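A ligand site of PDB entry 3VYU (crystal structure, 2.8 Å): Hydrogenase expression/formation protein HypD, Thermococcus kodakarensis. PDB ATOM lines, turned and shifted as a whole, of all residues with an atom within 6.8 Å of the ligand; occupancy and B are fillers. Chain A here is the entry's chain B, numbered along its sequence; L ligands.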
ATOM      1  N   LEU A 319     -22.816  11.968 -36.002  1.00  0.00           N
ATOM      2  CA  LEU A 319     -22.623  13.390 -35.719  1.00  0.00           C
ATOM      3  C   LEU A 319     -22.261  14.144 -36.992  1.00  0.00           C
ATOM      4  O   LEU A 319     -21.786  13.537 -37.957  1.00  0.00           O
ATOM      5  CB  LEU A 319     -21.501  13.572 -34.702  1.00  0.00           C
ATOM      6  CG  LEU A 319     -21.600  12.774 -33.396  1.00  0.00           C
ATOM      7  CD1 LEU A 319     -20.310  12.924 -32.609  1.00  0.00           C
ATOM      8  CD2 LEU A 319     -22.788  13.264 -32.588  1.00  0.00           C
ATOM      9  N   GLU A 320     -22.479  15.455 -36.999  1.00  0.00           N
ATOM     10  CA  GLU A 320     -22.130  16.254 -38.164  1.00  0.00           C
ATOM     11  C   GLU A 320     -20.630  16.547 -38.166  1.00  0.00           C
ATOM     12  O   GLU A 320     -20.000  16.596 -37.117  1.00  0.00           O
ATOM     13  CB  GLU A 320     -22.928  17.569 -38.174  1.00  0.00           C
ATOM     14  CG  GLU A 320     -24.350  17.409 -38.697  1.00  0.00           C
ATOM     15  CD  GLU A 320     -24.374  16.942 -40.144  1.00  0.00           C
ATOM     16  OE1 GLU A 320     -25.423  16.429 -40.588  1.00  0.00           O
ATOM     17  OE2 GLU A 320     -23.351  17.101 -40.847  1.00  0.00           O
ATOM     18  N   GLY A 322     -17.153  17.760 -37.746  1.00  0.00           N
ATOM     19  CA  GLY A 322     -16.629  18.729 -36.804  1.00  0.00           C
ATOM     20  C   GLY A 322     -16.964  18.510 -35.343  1.00  0.00           C
ATOM     21  O   GLY A 322     -16.226  18.924 -34.445  1.00  0.00           O
ATOM     22  N   CYS A 323     -18.095  17.846 -35.095  1.00  0.00           N
ATOM     23  CA  CYS A 323     -18.549  17.570 -33.730  1.00  0.00           C
ATOM     24  C   CYS A 323     -17.656  16.544 -33.042  1.00  0.00           C
ATOM     25  O   CYS A 323     -17.609  15.390 -33.449  1.00  0.00           O
ATOM     26  CB  CYS A 323     -19.991  17.047 -33.754  1.00  0.00           C
ATOM     27  SG  CYS A 323     -20.756  16.826 -32.109  1.00  0.00           S
ATOM     28  N   ARG A 324     -16.975  16.976 -31.981  1.00  0.00           N
ATOM     29  CA  ARG A 324     -16.099  16.089 -31.211  1.00  0.00           C
ATOM     30  C   ARG A 324     -16.815  15.611 -29.942  1.00  0.00           C
ATOM     31  O   ARG A 324     -16.184  15.414 -28.902  1.00  0.00           O
ATOM     32  CB  ARG A 324     -14.812  16.838 -30.839  1.00  0.00           C
ATOM     33  CG  ARG A 324     -13.893  17.133 -32.012  1.00  0.00           C
ATOM     34  CD  ARG A 324     -12.644  17.880 -31.564  1.00  0.00           C
ATOM     35  NE  ARG A 324     -11.938  17.156 -30.506  1.00  0.00           N
ATOM     36  CZ  ARG A 324     -10.828  17.583 -29.927  1.00  0.00           C
ATOM     37  NH1 ARG A 324     -10.282  18.733 -30.306  1.00  0.00           N
ATOM     38  NH2 ARG A 324     -10.249  16.867 -28.969  1.00  0.00           N
ATOM     39  N   CYS A 325     -18.132  15.423 -30.034  1.00  0.00           N
ATOM     40  CA  CYS A 325     -18.958  14.978 -28.920  1.00  0.00           C
ATOM     41  C   CYS A 325     -18.606  13.551 -28.500  1.00  0.00           C
ATOM     42  O   CYS A 325     -18.864  13.146 -27.364  1.00  0.00           O
ATOM     43  CB  CYS A 325     -20.449  15.100 -29.306  1.00  0.00           C
ATOM     44  SG  CYS A 325     -21.769  14.475 -28.190  1.00  0.00           S
ATOM     45  N   GLY A 326     -18.013  12.801 -29.425  1.00  0.00           N
ATOM     46  CA  GLY A 326     -17.628  11.437 -29.111  1.00  0.00           C
ATOM     47  C   GLY A 326     -16.490  11.444 -28.116  1.00  0.00           C
ATOM     48  O   GLY A 326     -16.452  10.619 -27.189  1.00  0.00           O
ATOM     49  N   VAL A 328     -15.913  13.910 -26.109  1.00  0.00           N
ATOM     50  CA  VAL A 328     -16.421  14.549 -24.898  1.00  0.00           C
ATOM     51  C   VAL A 328     -17.144  13.552 -23.997  1.00  0.00           C
ATOM     52  O   VAL A 328     -17.102  13.679 -22.776  1.00  0.00           O
ATOM     53  CB  VAL A 328     -17.385  15.696 -25.224  1.00  0.00           C
ATOM     54  CG1 VAL A 328     -17.877  16.333 -23.939  1.00  0.00           C
ATOM     55  CG2 VAL A 328     -16.685  16.724 -26.088  1.00  0.00           C
ATOM     56  N   PRO A 335     -15.761  20.235 -23.577  1.00  0.00           N
ATOM     57  CA  PRO A 335     -16.360  20.941 -24.714  1.00  0.00           C
ATOM     58  C   PRO A 335     -15.584  22.170 -25.178  1.00  0.00           C
ATOM     59  O   PRO A 335     -15.773  22.628 -26.301  1.00  0.00           O
ATOM     60  CB  PRO A 335     -17.768  21.259 -24.210  1.00  0.00           C
ATOM     61  CG  PRO A 335     -17.620  21.284 -22.721  1.00  0.00           C
ATOM     62  CD  PRO A 335     -16.707  20.130 -22.462  1.00  0.00           C
ATOM     63  N   ASP A 337     -12.533  22.149 -25.689  1.00  0.00           N
ATOM     64  CA  ASP A 337     -11.482  21.617 -26.553  1.00  0.00           C
ATOM     65  C   ASP A 337     -12.068  21.332 -27.936  1.00  0.00           C
ATOM     66  O   ASP A 337     -11.507  20.556 -28.707  1.00  0.00           O
ATOM     67  CB  ASP A 337     -10.894  20.321 -25.978  1.00  0.00           C
ATOM     68  CG  ASP A 337     -10.252  20.508 -24.619  1.00  0.00           C
ATOM     69  OD1 ASP A 337      -9.349  21.361 -24.489  1.00  0.00           O
ATOM     70  OD2 ASP A 337     -10.648  19.798 -23.674  1.00  0.00           O
ATOM     71  N   CYS A 338     -13.204  21.952 -28.221  1.00  0.00           N
ATOM     72  CA  CYS A 338     -13.874  21.760 -29.505  1.00  0.00           C
ATOM     73  C   CYS A 338     -13.934  23.039 -30.331  1.00  0.00           C
ATOM     74  O   CYS A 338     -14.456  24.068 -29.878  1.00  0.00           O
ATOM     75  CB  CYS A 338     -15.288  21.233 -29.292  1.00  0.00           C
ATOM     76  SG  CYS A 338     -16.308  21.307 -30.792  1.00  0.00           S
ATOM     77  N   PRO A 339     -13.425  22.992 -31.578  1.00  0.00           N
ATOM     78  CA  PRO A 339     -13.384  24.117 -32.520  1.00  0.00           C
ATOM     79  C   PRO A 339     -14.738  24.793 -32.802  1.00  0.00           C
ATOM     80  O   PRO A 339     -14.772  25.945 -33.237  1.00  0.00           O
ATOM     81  CB  PRO A 339     -12.784  23.487 -33.775  1.00  0.00           C
ATOM     82  CG  PRO A 339     -13.163  22.032 -33.648  1.00  0.00           C
ATOM     83  CD  PRO A 339     -12.891  21.778 -32.200  1.00  0.00           C
ATOM     84  N   LEU A 340     -15.830  24.086 -32.553  1.00  0.00           N
ATOM     85  CA  LEU A 340     -17.153  24.650 -32.798  1.00  0.00           C
ATOM     86  C   LEU A 340     -17.809  25.182 -31.529  1.00  0.00           C
ATOM     87  O   LEU A 340     -18.779  25.941 -31.597  1.00  0.00           O
ATOM     88  CB  LEU A 340     -18.064  23.609 -33.436  1.00  0.00           C
ATOM     89  CG  LEU A 340     -17.452  22.817 -34.598  1.00  0.00           C
ATOM     90  CD1 LEU A 340     -18.493  21.874 -35.154  1.00  0.00           C
ATOM     91  CD2 LEU A 340     -16.959  23.769 -35.671  1.00  0.00           C
ATOM     92  N   PHE A 341     -17.300  24.769 -30.369  1.00  0.00           N
ATOM     93  CA  PHE A 341     -17.887  25.203 -29.113  1.00  0.00           C
ATOM     94  C   PHE A 341     -17.940  26.723 -28.928  1.00  0.00           C
ATOM     95  O   PHE A 341     -16.902  27.387 -28.898  1.00  0.00           O
ATOM     96  CB  PHE A 341     -17.146  24.609 -27.924  1.00  0.00           C
ATOM     97  CG  PHE A 341     -17.693  25.063 -26.618  1.00  0.00           C
ATOM     98  CD1 PHE A 341     -18.980  24.709 -26.227  1.00  0.00           C
ATOM     99  CD2 PHE A 341     -16.975  25.941 -25.823  1.00  0.00           C
ATOM    100  CE1 PHE A 341     -19.528  25.206 -25.055  1.00  0.00           C
ATOM    101  CE2 PHE A 341     -17.519  26.447 -24.647  1.00  0.00           C
ATOM    102  CZ  PHE A 341     -18.800  26.081 -24.262  1.00  0.00           C
ATOM    103  N   GLY A 342     -19.149  27.244 -28.772  1.00  0.00           N
ATOM    104  CA  GLY A 342     -19.343  28.665 -28.558  1.00  0.00           C
ATOM    105  C   GLY A 342     -19.356  29.472 -29.843  1.00  0.00           C
ATOM    106  O   GLY A 342     -19.634  30.670 -29.820  1.00  0.00           O
ATOM    107  N   THR A 344     -20.067  28.054 -33.866  1.00  0.00           N
ATOM    108  CA  THR A 344     -21.105  27.523 -34.733  1.00  0.00           C
ATOM    109  C   THR A 344     -22.054  26.650 -33.931  1.00  0.00           C
ATOM    110  O   THR A 344     -23.197  26.438 -34.337  1.00  0.00           O
ATOM    111  CB  THR A 344     -20.474  26.667 -35.848  1.00  0.00           C
ATOM    112  OG1 THR A 344     -20.405  25.304 -35.430  1.00  0.00           O
ATOM    113  CG2 THR A 344     -19.060  27.157 -36.142  1.00  0.00           C
ATOM    114  N   CYS A 345     -21.593  26.152 -32.795  1.00  0.00           N
ATOM    115  CA  CYS A 345     -22.416  25.300 -31.957  1.00  0.00           C
ATOM    116  C   CYS A 345     -22.764  25.938 -30.613  1.00  0.00           C
ATOM    117  O   CYS A 345     -21.898  26.213 -29.783  1.00  0.00           O
ATOM    118  CB  CYS A 345     -21.698  23.961 -31.714  1.00  0.00           C
ATOM    119  SG  CYS A 345     -22.646  22.721 -30.765  1.00  0.00           S
ATOM    120  N   THR A 346     -24.056  26.167 -30.426  1.00  0.00           N
ATOM    121  CA  THR A 346     -24.586  26.740 -29.200  1.00  0.00           C
ATOM    122  C   THR A 346     -25.976  26.165 -29.043  1.00  0.00           C
ATOM    123  O   THR A 346     -26.534  25.594 -29.995  1.00  0.00           O
ATOM    124  CB  THR A 346     -24.682  28.271 -29.281  1.00  0.00           C
ATOM    125  OG1 THR A 346     -25.641  28.627 -30.301  1.00  0.00           O
ATOM    126  CG2 THR A 346     -23.329  28.879 -29.619  1.00  0.00           C
ATOM    127  N   PRO A 350     -27.395  24.244 -32.320  1.00  0.00           N
ATOM    128  CA  PRO A 350     -26.475  23.152 -31.991  1.00  0.00           C
ATOM    129  C   PRO A 350     -26.087  22.276 -33.178  1.00  0.00           C
ATOM    130  O   PRO A 350     -26.819  22.181 -34.166  1.00  0.00           O
ATOM    131  CB  PRO A 350     -27.263  22.369 -30.961  1.00  0.00           C
ATOM    132  CG  PRO A 350     -28.648  22.460 -31.507  1.00  0.00           C
ATOM    133  CD  PRO A 350     -28.763  23.914 -31.894  1.00  0.00           C
ATOM    134  N   VAL A 351     -24.930  21.628 -33.050  1.00  0.00           N
ATOM    135  CA  VAL A 351     -24.416  20.733 -34.077  1.00  0.00           C
ATOM    136  C   VAL A 351     -24.555  19.283 -33.610  1.00  0.00           C
ATOM    137  O   VAL A 351     -25.090  18.437 -34.323  1.00  0.00           O
ATOM    138  CB  VAL A 351     -22.916  21.007 -34.349  1.00  0.00           C
ATOM    139  CG1 VAL A 351     -22.385  20.002 -35.360  1.00  0.00           C
ATOM    140  CG2 VAL A 351     -22.735  22.422 -34.866  1.00  0.00           C
ATOM    141  N   GLY A 352     -24.067  19.017 -32.407  1.00  0.00           N
ATOM    142  CA  GLY A 352     -24.148  17.670 -31.855  1.00  0.00           C
ATOM    143  C   GLY A 352     -25.099  17.597 -30.670  1.00  0.00           C
ATOM    144  O   GLY A 352     -25.466  18.625 -30.106  1.00  0.00           O
ATOM    145  N   PRO A 353     -25.523  16.382 -30.272  1.00  0.00           N
ATOM    146  CA  PRO A 353     -26.445  16.188 -29.142  1.00  0.00           C
ATOM    147  C   PRO A 353     -25.905  16.691 -27.803  1.00  0.00           C
ATOM    148  O   PRO A 353     -26.654  17.128 -26.942  1.00  0.00           O
ATOM    149  CB  PRO A 353     -26.676  14.684 -29.153  1.00  0.00           C
ATOM    150  CG  PRO A 353     -25.389  14.149 -29.680  1.00  0.00           C
ATOM    151  CD  PRO A 353     -25.080  15.085 -30.816  1.00  0.00           C
ATOM    152  N   CYS A 354     -24.588  16.618 -27.650  1.00  0.00           N
ATOM    153  CA  CYS A 354     -23.928  17.078 -26.434  1.00  0.00           C
ATOM    154  C   CYS A 354     -24.338  18.499 -26.056  1.00  0.00           C
ATOM    155  O   CYS A 354     -24.147  18.921 -24.921  1.00  0.00           O
ATOM    156  CB  CYS A 354     -22.406  17.052 -26.631  1.00  0.00           C
ATOM    157  SG  CYS A 354     -21.529  15.465 -26.427  1.00  0.00           S
ATOM    158  N   MET A 355     -24.886  19.238 -27.017  1.00  0.00           N
ATOM    159  CA  MET A 355     -25.283  20.622 -26.765  1.00  0.00           C
ATOM    160  C   MET A 355     -26.805  20.762 -26.672  1.00  0.00           C
ATOM    161  O   MET A 355     -27.308  21.821 -26.283  1.00  0.00           O
ATOM    162  CB  MET A 355     -24.746  21.515 -27.888  1.00  0.00           C
ATOM    163  CG  MET A 355     -24.892  23.029 -27.668  1.00  0.00           C
ATOM    164  SD  MET A 355     -23.745  23.730 -26.448  1.00  0.00           S
ATOM    165  CE  MET A 355     -22.312  24.101 -27.450  1.00  0.00           C
ATOM    166  N   VAL A 356     -27.516  19.707 -27.020  1.00  0.00           N
ATOM    167  CA  VAL A 356     -28.977  19.720 -26.974  1.00  0.00           C
ATOM    168  C   VAL A 356     -29.549  19.169 -25.667  1.00  0.00           C
ATOM    169  O   VAL A 356     -30.396  19.799 -25.044  1.00  0.00           O
ATOM    170  CB  VAL A 356     -29.577  18.895 -28.122  1.00  0.00           C
ATOM    171  CG1 VAL A 356     -31.092  18.921 -28.046  1.00  0.00           C
ATOM    172  CG2 VAL A 356     -29.099  19.444 -29.458  1.00  0.00           C
ATOM    173  N   THR A 361     -22.795  17.572 -21.601  1.00  0.00           N
ATOM    174  CA  THR A 361     -21.607  18.238 -21.087  1.00  0.00           C
ATOM    175  C   THR A 361     -21.372  19.594 -21.752  1.00  0.00           C
ATOM    176  O   THR A 361     -20.921  20.540 -21.100  1.00  0.00           O
ATOM    177  CB  THR A 361     -20.345  17.368 -21.289  1.00  0.00           C
ATOM    178  OG1 THR A 361     -20.475  16.150 -20.536  1.00  0.00           O
ATOM    179  CG2 THR A 361     -19.101  18.119 -20.817  1.00  0.00           C
ATOM    180  N   CYS A 362     -21.684  19.682 -23.041  1.00  0.00           N
ATOM    181  CA  CYS A 362     -21.502  20.920 -23.789  1.00  0.00           C
ATOM    182  C   CYS A 362     -22.527  21.986 -23.447  1.00  0.00           C
ATOM    183  O   CYS A 362     -22.179  23.167 -23.332  1.00  0.00           O
ATOM    184  CB  CYS A 362     -21.535  20.632 -25.288  1.00  0.00           C
ATOM    185  SG  CYS A 362     -20.252  19.459 -25.810  1.00  0.00           S
ATOM    186  N   GLN A 363     -23.794  21.590 -23.294  1.00  0.00           N
ATOM    187  CA  GLN A 363     -24.843  22.544 -22.968  1.00  0.00           C
ATOM    188  C   GLN A 363     -24.578  23.144 -21.606  1.00  0.00           C
ATOM    189  O   GLN A 363     -24.906  24.303 -21.346  1.00  0.00           O
ATOM    190  CB  GLN A 363     -26.216  21.879 -22.927  1.00  0.00           C
ATOM    191  CG  GLN A 363     -27.330  22.834 -22.499  1.00  0.00           C
ATOM    192  CD  GLN A 363     -28.705  22.193 -22.513  1.00  0.00           C
ATOM    193  OE1 GLN A 363     -29.052  21.476 -23.441  1.00  0.00           O
ATOM    194  NE2 GLN A 363     -29.493  22.457 -21.474  1.00  0.00           N
HETATM  195 FE1  LIG L   1     -20.289  18.581 -30.657  1.00  0.00          FE
HETATM  196 FE2  LIG L   1     -21.110  21.101 -30.238  1.00  0.00          FE
HETATM  197 FE3  LIG L   1     -18.335  20.598 -30.061  1.00  0.00          FE
HETATM  198 FE4  LIG L   1     -19.912  19.767 -28.007  1.00  0.00          FE
HETATM  199  S1  LIG L   1     -19.876  21.792 -28.808  1.00  0.00           S
HETATM  200  S2  LIG L   1     -18.686  18.391 -29.433  1.00  0.00           S
HETATM  201  S3  LIG L   1     -21.949  19.601 -29.387  1.00  0.00           S
HETATM  202  S4  LIG L   1     -20.071  20.596 -31.755  1.00  0.00           S
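A sulfur (S2) of the ligand sits close to the backbone NH (N) of Cys 325, at 3.1 Å. SG of Cys 345 binds FE2 of the ligand (2.3 Å). A sulfur (S3) of the ligand lies close to the backbone NH (N) of Gly 352, at 3.7 Å. A sulfur (S2) of the ligand sits close to the backbone NH of Arg 324 (3.4 Å). FE3 of the ligand is bound by SG of Cys 338, 2.3 Å away. SG of Cys 323 is bound to FE1 of the ligand (2.3 Å). The side-chain sulfur (SG) of Cys 362 binds an iron atom (FE4) of the ligand, 2.2 Å away. S3 of the ligand lies close to N of Met 355.
The side-chain sulfur of Cys 345 lies close to the backbone NH of Val 351, at 3.4 Å. The guanidinium group (NH1) of Arg 324 lies within hydrogen-bond range of the backbone carbonyl oxygen (O) of Asp 337, 2.7 Å away. OE1 of Gln 363 lies close to O of Met 355, 3.4 Å away. SG of Cys 338 sits close to N of Phe 341. SG of Cys 325 is disulfide-bonded to SG of Cys 354. N of Cys 362 sits close to O of Cys 354, 3.2 Å away. N of Gln 363 sits at hydrogen-bond distance from O of Cys 354, at 3.1 Å. The backbone NH of Cys 345 is in hydrogen-bond range of the backbone carbonyl oxygen of Leu 340, at 3.1 Å.
CD1 of Leu 340 touches S4 of the ligand, 3.96 Å away. Phe 341 touches the ligand (CA to S1, 3.96 Å). Val 351 touches the ligand (CB to S4, 3.9 Å). Cys 354 touches the ligand (CB to S3, 3.8 Å). Hydrophobic or aromatic side chains that line the ligand: Leu 340, Phe 341, Val 351 and Met 355. The nearest printed residue that does not touch the ligand is Val 328 (4.2 Å).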
